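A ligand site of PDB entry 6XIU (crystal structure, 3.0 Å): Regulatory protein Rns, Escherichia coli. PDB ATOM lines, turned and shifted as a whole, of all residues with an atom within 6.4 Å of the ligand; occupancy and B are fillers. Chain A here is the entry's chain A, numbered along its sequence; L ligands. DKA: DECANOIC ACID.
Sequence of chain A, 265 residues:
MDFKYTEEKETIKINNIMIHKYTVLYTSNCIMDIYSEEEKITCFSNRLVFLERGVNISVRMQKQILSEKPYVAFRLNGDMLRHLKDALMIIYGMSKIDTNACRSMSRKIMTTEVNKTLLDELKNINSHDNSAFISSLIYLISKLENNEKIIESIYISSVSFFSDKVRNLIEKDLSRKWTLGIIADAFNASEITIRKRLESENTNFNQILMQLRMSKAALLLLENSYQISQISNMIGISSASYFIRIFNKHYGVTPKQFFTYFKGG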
ATOM      1  N   ILE A  14     -19.061  -5.548   5.552  1.00  0.00           N
ATOM      2  CA  ILE A  14     -19.416  -6.695   4.718  1.00  0.00           C
ATOM      3  C   ILE A  14     -18.130  -7.190   4.058  1.00  0.00           C
ATOM      4  O   ILE A  14     -17.439  -6.433   3.376  1.00  0.00           O
ATOM      5  CB  ILE A  14     -20.477  -6.328   3.669  1.00  0.00           C
ATOM      6  CG1 ILE A  14     -21.609  -5.550   4.314  1.00  0.00           C
ATOM      7  CG2 ILE A  14     -21.055  -7.578   3.018  1.00  0.00           C
ATOM      8  CD1 ILE A  14     -22.785  -5.415   3.393  1.00  0.00           C
ATOM      9  N   ILE A  17     -17.036  -9.566  -0.625  1.00  0.00           N
ATOM     10  CA  ILE A  17     -17.944  -9.324  -1.740  1.00  0.00           C
ATOM     11  C   ILE A  17     -17.180  -9.459  -3.051  1.00  0.00           C
ATOM     12  O   ILE A  17     -16.271  -8.675  -3.340  1.00  0.00           O
ATOM     13  CB  ILE A  17     -18.574  -7.925  -1.636  1.00  0.00           C
ATOM     14  CG1 ILE A  17     -19.087  -7.673  -0.246  1.00  0.00           C
ATOM     15  CG2 ILE A  17     -19.713  -7.830  -2.587  1.00  0.00           C
ATOM     16  CD1 ILE A  17     -19.269  -6.241  -0.040  1.00  0.00           C
ATOM     17  N   MET A  18     -17.643 -10.356  -3.917  1.00  0.00           N
ATOM     18  CA  MET A  18     -16.951 -10.714  -5.140  1.00  0.00           C
ATOM     19  C   MET A  18     -17.797 -10.290  -6.328  1.00  0.00           C
ATOM     20  O   MET A  18     -18.960 -10.680  -6.447  1.00  0.00           O
ATOM     21  CB  MET A  18     -16.694 -12.209  -5.212  1.00  0.00           C
ATOM     22  CG  MET A  18     -16.686 -12.762  -6.617  1.00  0.00           C
ATOM     23  SD  MET A  18     -15.112 -12.730  -7.381  1.00  0.00           S
ATOM     24  CE  MET A  18     -14.123 -13.746  -6.228  1.00  0.00           C
ATOM     25  N   ILE A  19     -17.204  -9.491  -7.213  1.00  0.00           N
ATOM     26  CA  ILE A  19     -17.929  -8.803  -8.271  1.00  0.00           C
ATOM     27  C   ILE A  19     -17.902  -9.678  -9.524  1.00  0.00           C
ATOM     28  O   ILE A  19     -16.857  -9.908 -10.123  1.00  0.00           O
ATOM     29  CB  ILE A  19     -17.326  -7.408  -8.526  1.00  0.00           C
ATOM     30  CG1 ILE A  19     -17.824  -6.392  -7.484  1.00  0.00           C
ATOM     31  CG2 ILE A  19     -17.580  -6.978  -9.935  1.00  0.00           C
ATOM     32  CD1 ILE A  19     -17.221  -6.501  -6.135  1.00  0.00           C
ATOM     33  N   HIS A  20     -19.074 -10.183  -9.894  1.00  0.00           N
ATOM     34  CA  HIS A  20     -19.269 -11.112 -10.999  1.00  0.00           C
ATOM     35  C   HIS A  20     -19.649 -10.422 -12.267  1.00  0.00           C
ATOM     36  O   HIS A  20     -19.746 -11.081 -13.312  1.00  0.00           O
ATOM     37  CB  HIS A  20     -20.398 -12.070 -10.694  1.00  0.00           C
ATOM     38  CG  HIS A  20     -20.115 -12.928  -9.523  1.00  0.00           C
ATOM     39  ND1 HIS A  20     -20.374 -12.510  -8.229  1.00  0.00           N
ATOM     40  CD2 HIS A  20     -19.563 -14.159  -9.448  1.00  0.00           C
ATOM     41  CE1 HIS A  20     -19.974 -13.469  -7.411  1.00  0.00           C
ATOM     42  NE2 HIS A  20     -19.498 -14.476  -8.124  1.00  0.00           N
ATOM     43  N   LYS A  21     -19.906  -9.126 -12.189  1.00  0.00           N
ATOM     44  CA  LYS A  21     -20.343  -8.305 -13.285  1.00  0.00           C
ATOM     45  C   LYS A  21     -19.707  -6.955 -13.083  1.00  0.00           C
ATOM     46  O   LYS A  21     -19.750  -6.421 -11.979  1.00  0.00           O
ATOM     47  CB  LYS A  21     -21.857  -8.131 -13.292  1.00  0.00           C
ATOM     48  CG  LYS A  21     -22.606  -9.390 -13.564  1.00  0.00           C
ATOM     49  CD  LYS A  21     -24.107  -9.235 -13.371  1.00  0.00           C
ATOM     50  CE  LYS A  21     -24.803 -10.510 -13.797  1.00  0.00           C
ATOM     51  NZ  LYS A  21     -26.214 -10.442 -13.437  1.00  0.00           N
ATOM     52  N   THR A  23     -19.289  -3.425 -12.435  1.00  0.00           N
ATOM     53  CA  THR A  23     -20.253  -2.701 -11.612  1.00  0.00           C
ATOM     54  C   THR A  23     -19.950  -1.211 -11.571  1.00  0.00           C
ATOM     55  O   THR A  23     -18.788  -0.815 -11.400  1.00  0.00           O
ATOM     56  CB  THR A  23     -20.281  -3.219 -10.191  1.00  0.00           C
ATOM     57  OG1 THR A  23     -20.765  -4.577 -10.180  1.00  0.00           O
ATOM     58  CG2 THR A  23     -21.141  -2.310  -9.313  1.00  0.00           C
ATOM     59  N   LEU A  25     -21.122   2.070  -9.432  1.00  0.00           N
ATOM     60  CA  LEU A  25     -21.794   2.331  -8.164  1.00  0.00           C
ATOM     61  C   LEU A  25     -21.834   3.841  -7.984  1.00  0.00           C
ATOM     62  O   LEU A  25     -20.871   4.521  -8.291  1.00  0.00           O
ATOM     63  CB  LEU A  25     -21.047   1.635  -7.036  1.00  0.00           C
ATOM     64  CG  LEU A  25     -21.851   1.173  -5.816  1.00  0.00           C
ATOM     65  CD1 LEU A  25     -21.091   0.057  -5.171  1.00  0.00           C
ATOM     66  CD2 LEU A  25     -22.039   2.297  -4.857  1.00  0.00           C
ATOM     67  N   MET A  32     -17.956   5.244   2.072  1.00  0.00           N
ATOM     68  CA  MET A  32     -17.637   3.816   2.066  1.00  0.00           C
ATOM     69  C   MET A  32     -16.138   3.573   1.928  1.00  0.00           C
ATOM     70  O   MET A  32     -15.487   4.205   1.106  1.00  0.00           O
ATOM     71  CB  MET A  32     -18.441   3.130   0.946  1.00  0.00           C
ATOM     72  CG  MET A  32     -17.857   1.890   0.298  1.00  0.00           C
ATOM     73  SD  MET A  32     -18.919   1.382  -1.083  1.00  0.00           S
ATOM     74  CE  MET A  32     -18.834   2.822  -2.099  1.00  0.00           C
ATOM     75  N   LEU A  51     -16.031  -0.649 -10.612  1.00  0.00           N
ATOM     76  CA  LEU A  51     -15.570  -1.867  -9.966  1.00  0.00           C
ATOM     77  C   LEU A  51     -15.328  -2.885 -11.067  1.00  0.00           C
ATOM     78  O   LEU A  51     -16.278  -3.321 -11.750  1.00  0.00           O
ATOM     79  CB  LEU A  51     -16.594  -2.374  -8.951  1.00  0.00           C
ATOM     80  CG  LEU A  51     -16.909  -1.355  -7.870  1.00  0.00           C
ATOM     81  CD1 LEU A  51     -18.267  -1.564  -7.321  1.00  0.00           C
ATOM     82  CD2 LEU A  51     -15.905  -1.430  -6.756  1.00  0.00           C
ATOM     83  N   ILE A  57     -13.664  -7.713  -2.699  1.00  0.00           N
ATOM     84  CA  ILE A  57     -13.413  -6.535  -1.894  1.00  0.00           C
ATOM     85  C   ILE A  57     -14.143  -6.692  -0.567  1.00  0.00           C
ATOM     86  O   ILE A  57     -14.974  -7.569  -0.412  1.00  0.00           O
ATOM     87  CB  ILE A  57     -13.858  -5.244  -2.581  1.00  0.00           C
ATOM     88  CG1 ILE A  57     -15.382  -5.284  -2.766  1.00  0.00           C
ATOM     89  CG2 ILE A  57     -13.215  -5.147  -3.905  1.00  0.00           C
ATOM     90  CD1 ILE A  57     -15.965  -3.963  -3.187  1.00  0.00           C
ATOM     91  N   VAL A  59     -15.999  -4.021   2.554  1.00  0.00           N
ATOM     92  CA  VAL A  59     -16.644  -2.704   2.532  1.00  0.00           C
ATOM     93  C   VAL A  59     -17.071  -2.327   3.935  1.00  0.00           C
ATOM     94  O   VAL A  59     -17.699  -3.127   4.634  1.00  0.00           O
ATOM     95  CB  VAL A  59     -17.889  -2.681   1.607  1.00  0.00           C
ATOM     96  CG1 VAL A  59     -18.577  -1.340   1.674  1.00  0.00           C
ATOM     97  CG2 VAL A  59     -17.515  -2.974   0.171  1.00  0.00           C
ATOM     98  N   MET A  61     -19.361   0.745   5.388  1.00  0.00           N
ATOM     99  CA  MET A  61     -20.127   1.811   4.736  1.00  0.00           C
ATOM    100  C   MET A  61     -21.149   2.393   5.692  1.00  0.00           C
ATOM    101  O   MET A  61     -21.757   1.664   6.478  1.00  0.00           O
ATOM    102  CB  MET A  61     -20.794   1.329   3.427  1.00  0.00           C
ATOM    103  CG  MET A  61     -22.307   1.108   3.450  1.00  0.00           C
ATOM    104  SD  MET A  61     -22.976   0.468   1.883  1.00  0.00           S
ATOM    105  CE  MET A  61     -22.279  -1.179   1.815  1.00  0.00           C
ATOM    106  N   TYR A  71     -26.847   3.290  -1.726  1.00  0.00           N
ATOM    107  CA  TYR A  71     -26.237   3.694  -2.969  1.00  0.00           C
ATOM    108  C   TYR A  71     -27.153   3.267  -4.098  1.00  0.00           C
ATOM    109  O   TYR A  71     -28.247   2.741  -3.873  1.00  0.00           O
ATOM    110  CB  TYR A  71     -24.870   3.049  -3.132  1.00  0.00           C
ATOM    111  CG  TYR A  71     -24.942   1.532  -3.048  1.00  0.00           C
ATOM    112  CD1 TYR A  71     -25.369   0.785  -4.118  1.00  0.00           C
ATOM    113  CD2 TYR A  71     -24.533   0.856  -1.920  1.00  0.00           C
ATOM    114  CE1 TYR A  71     -25.442  -0.578  -4.054  1.00  0.00           C
ATOM    115  CE2 TYR A  71     -24.590  -0.521  -1.860  1.00  0.00           C
ATOM    116  CZ  TYR A  71     -25.060  -1.232  -2.939  1.00  0.00           C
ATOM    117  OH  TYR A  71     -25.132  -2.598  -2.910  1.00  0.00           O
ATOM    118  N   ARG A  75     -25.173  -3.103 -12.893  1.00  0.00           N
ATOM    119  CA  ARG A  75     -24.368  -4.292 -13.121  1.00  0.00           C
ATOM    120  C   ARG A  75     -24.539  -4.734 -14.559  1.00  0.00           C
ATOM    121  O   ARG A  75     -25.656  -5.013 -14.994  1.00  0.00           O
ATOM    122  CB  ARG A  75     -24.788  -5.419 -12.172  1.00  0.00           C
ATOM    123  CG  ARG A  75     -24.816  -5.037 -10.700  1.00  0.00           C
ATOM    124  CD  ARG A  75     -25.801  -5.853  -9.859  1.00  0.00           C
ATOM    125  NE  ARG A  75     -25.789  -7.284 -10.123  1.00  0.00           N
ATOM    126  CZ  ARG A  75     -24.718  -8.085 -10.019  1.00  0.00           C
ATOM    127  NH1 ARG A  75     -23.529  -7.583  -9.672  1.00  0.00           N
ATOM    128  NH2 ARG A  75     -24.845  -9.387 -10.253  1.00  0.00           N
ATOM    129  N   GLN A 211     -18.559 -18.374  -3.653  1.00  0.00           N
ATOM    130  CA  GLN A 211     -18.853 -17.011  -4.111  1.00  0.00           C
ATOM    131  C   GLN A 211     -20.106 -16.941  -4.994  1.00  0.00           C
ATOM    132  O   GLN A 211     -20.878 -15.971  -4.901  1.00  0.00           O
ATOM    133  CB  GLN A 211     -17.655 -16.430  -4.860  1.00  0.00           C
ATOM    134  CG  GLN A 211     -16.360 -16.221  -4.094  1.00  0.00           C
ATOM    135  CD  GLN A 211     -16.386 -15.087  -3.102  1.00  0.00           C
ATOM    136  OE1 GLN A 211     -17.408 -14.398  -2.933  1.00  0.00           O
ATOM    137  NE2 GLN A 211     -15.228 -14.835  -2.472  1.00  0.00           N
ATOM    138  N   MET A 214     -23.079 -17.380  -2.504  1.00  0.00           N
ATOM    139  CA  MET A 214     -23.284 -16.272  -1.572  1.00  0.00           C
ATOM    140  C   MET A 214     -23.687 -14.985  -2.298  1.00  0.00           C
ATOM    141  O   MET A 214     -24.493 -14.209  -1.771  1.00  0.00           O
ATOM    142  CB  MET A 214     -22.017 -16.096  -0.717  1.00  0.00           C
ATOM    143  CG  MET A 214     -21.834 -17.148   0.393  1.00  0.00           C
ATOM    144  SD  MET A 214     -23.270 -17.353   1.496  1.00  0.00           S
ATOM    145  CE  MET A 214     -24.038 -18.807   0.789  1.00  0.00           C
ATOM    146  N   SER A 215     -23.206 -14.745  -3.530  1.00  0.00           N
ATOM    147  CA  SER A 215     -23.716 -13.623  -4.308  1.00  0.00           C
ATOM    148  C   SER A 215     -25.170 -13.818  -4.679  1.00  0.00           C
ATOM    149  O   SER A 215     -25.988 -12.910  -4.507  1.00  0.00           O
ATOM    150  CB  SER A 215     -22.893 -13.457  -5.575  1.00  0.00           C
ATOM    151  OG  SER A 215     -21.570 -13.162  -5.182  1.00  0.00           O
ATOM    152  N   ALA A 218     -27.263 -13.164  -1.736  1.00  0.00           N
ATOM    153  CA  ALA A 218     -27.401 -11.750  -1.405  1.00  0.00           C
ATOM    154  C   ALA A 218     -28.434 -11.081  -2.318  1.00  0.00           C
ATOM    155  O   ALA A 218     -29.373 -10.418  -1.843  1.00  0.00           O
ATOM    156  CB  ALA A 218     -26.043 -11.055  -1.522  1.00  0.00           C
ATOM    157  N   LEU A 219     -28.297 -11.269  -3.643  1.00  0.00           N
ATOM    158  CA  LEU A 219     -29.195 -10.644  -4.601  1.00  0.00           C
ATOM    159  C   LEU A 219     -30.649 -11.062  -4.366  1.00  0.00           C
ATOM    160  O   LEU A 219     -31.580 -10.231  -4.306  1.00  0.00           O
ATOM    161  CB  LEU A 219     -28.761 -11.052  -6.013  1.00  0.00           C
ATOM    162  CG  LEU A 219     -27.369 -10.599  -6.450  1.00  0.00           C
ATOM    163  CD1 LEU A 219     -26.874 -11.388  -7.646  1.00  0.00           C
ATOM    164  CD2 LEU A 219     -27.445  -9.161  -6.768  1.00  0.00           C
ATOM    165  N   LEU A 222     -32.159  -9.439  -1.518  1.00  0.00           N
ATOM    166  CA  LEU A 222     -32.536  -8.046  -1.766  1.00  0.00           C
ATOM    167  C   LEU A 222     -33.835  -7.914  -2.540  1.00  0.00           C
ATOM    168  O   LEU A 222     -34.494  -6.871  -2.450  1.00  0.00           O
ATOM    169  CB  LEU A 222     -31.423  -7.319  -2.508  1.00  0.00           C
ATOM    170  CG  LEU A 222     -30.155  -7.147  -1.687  1.00  0.00           C
ATOM    171  CD1 LEU A 222     -28.999  -6.640  -2.495  1.00  0.00           C
ATOM    172  CD2 LEU A 222     -30.514  -6.136  -0.647  1.00  0.00           C
ATOM    173  N   TYR A 251     -20.127 -13.285   4.840  1.00  0.00           N
ATOM    174  CA  TYR A 251     -20.276 -11.855   4.636  1.00  0.00           C
ATOM    175  C   TYR A 251     -19.971 -11.052   5.882  1.00  0.00           C
ATOM    176  O   TYR A 251     -19.718  -9.850   5.768  1.00  0.00           O
ATOM    177  CB  TYR A 251     -21.681 -11.498   4.111  1.00  0.00           C
ATOM    178  CG  TYR A 251     -21.846 -11.726   2.608  1.00  0.00           C
ATOM    179  CD1 TYR A 251     -21.358 -10.819   1.692  1.00  0.00           C
ATOM    180  CD2 TYR A 251     -22.525 -12.838   2.104  1.00  0.00           C
ATOM    181  CE1 TYR A 251     -21.498 -11.012   0.354  1.00  0.00           C
ATOM    182  CE2 TYR A 251     -22.674 -13.045   0.761  1.00  0.00           C
ATOM    183  CZ  TYR A 251     -22.162 -12.122  -0.120  1.00  0.00           C
ATOM    184  OH  TYR A 251     -22.276 -12.291  -1.494  1.00  0.00           O
ATOM    185  N   PHE A 258     -28.156  -7.924   6.919  1.00  0.00           N
ATOM    186  CA  PHE A 258     -27.912  -7.481   5.546  1.00  0.00           C
ATOM    187  C   PHE A 258     -29.179  -6.904   4.930  1.00  0.00           C
ATOM    188  O   PHE A 258     -29.208  -5.739   4.510  1.00  0.00           O
ATOM    189  CB  PHE A 258     -27.401  -8.695   4.761  1.00  0.00           C
ATOM    190  CG  PHE A 258     -27.129  -8.415   3.339  1.00  0.00           C
ATOM    191  CD1 PHE A 258     -25.864  -8.053   2.942  1.00  0.00           C
ATOM    192  CD2 PHE A 258     -28.121  -8.539   2.383  1.00  0.00           C
ATOM    193  CE1 PHE A 258     -25.592  -7.801   1.605  1.00  0.00           C
ATOM    194  CE2 PHE A 258     -27.860  -8.279   1.044  1.00  0.00           C
ATOM    195  CZ  PHE A 258     -26.591  -7.911   0.641  1.00  0.00           C
ATOM    196  N   PHE A 262     -30.106  -2.964   3.838  1.00  0.00           N
ATOM    197  CA  PHE A 262     -30.225  -2.516   2.448  1.00  0.00           C
ATOM    198  C   PHE A 262     -31.657  -2.178   2.011  1.00  0.00           C
ATOM    199  O   PHE A 262     -31.813  -1.526   0.979  1.00  0.00           O
ATOM    200  CB  PHE A 262     -29.633  -3.570   1.499  1.00  0.00           C
ATOM    201  CG  PHE A 262     -28.134  -3.493   1.367  1.00  0.00           C
ATOM    202  CD1 PHE A 262     -27.550  -2.680   0.393  1.00  0.00           C
ATOM    203  CD2 PHE A 262     -27.301  -4.209   2.233  1.00  0.00           C
ATOM    204  CE1 PHE A 262     -26.160  -2.592   0.256  1.00  0.00           C
ATOM    205  CE2 PHE A 262     -25.902  -4.139   2.132  1.00  0.00           C
ATOM    206  CZ  PHE A 262     -25.316  -3.329   1.124  1.00  0.00           C
HETATM  207  C1  DKA L   1     -21.950  -9.343  -6.897  1.00  0.00           C
HETATM  208  O1  DKA L   1     -22.267  -8.307  -7.529  1.00  0.00           O
HETATM  209  C2  DKA L   1     -22.267  -9.459  -5.405  1.00  0.00           C
HETATM  210  C3  DKA L   1     -23.260  -8.390  -4.939  1.00  0.00           C
HETATM  211  C4  DKA L   1     -23.494  -8.437  -3.428  1.00  0.00           C
HETATM  212  C5  DKA L   1     -22.736  -7.342  -2.694  1.00  0.00           C
HETATM  213  C6  DKA L   1     -23.653  -6.508  -1.804  1.00  0.00           C
HETATM  214  C7  DKA L   1     -22.903  -5.386  -1.079  1.00  0.00           C
HETATM  215  C8  DKA L   1     -21.873  -4.719  -1.975  1.00  0.00           C
HETATM  216  C9  DKA L   1     -22.052  -3.196  -2.026  1.00  0.00           C
HETATM  217  C10 DKA L   1     -20.723  -2.461  -2.188  1.00  0.00           C
HETATM  218  O2  DKA L   1     -21.370 -10.300  -7.484  1.00  0.00           O
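O2 of the ligand sits at hydrogen-bond distance from N of His 20 (3.3 Å). An oxygen (O2) of the ligand lies within hydrogen-bond range of a ring nitrogen (ND1) of His 20 (2.5 Å). An oxygen (O1) of the ligand is in salt-bridge range of the guanidinium group of Arg 75, 2.6 Å away. O of Met 18 lies close to O2 of the ligand (2.7 Å).
ND1 of His 20 sits at hydrogen-bond distance from O of Met 18, at 2.9 Å. ND1 of His 20 lies close to OG of Ser 215, 3.3 Å away. The backbone carbonyl oxygen (O) of Ile 17 lies within hydrogen-bond range of the backbone NH (N) of Ile 57, at 2.9 Å. The backbone NH of Ser 215 sits at hydrogen-bond distance from the side-chain hydroxyl of Tyr 251 (3.3 Å). OG of Ser 215 lies within hydrogen-bond range of O of Gln 211, 2.9 Å away.
Ile 17 touches the ligand. CA of Ile 19 touches O2 of the ligand, 3.8 Å away. Leu 25 touches the ligand. OH of Tyr 71 touches C9 of the ligand, 3.3 Å away. Ser 215 touches the ligand. Phe 262 touches the ligand (CZ to C7, 3.9 Å). Within 4 Å of the ligand: Ile 17, Met 18, Ile 19, His 20, Leu 25, Tyr 71, Arg 75, Ser 215 and Phe 262.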
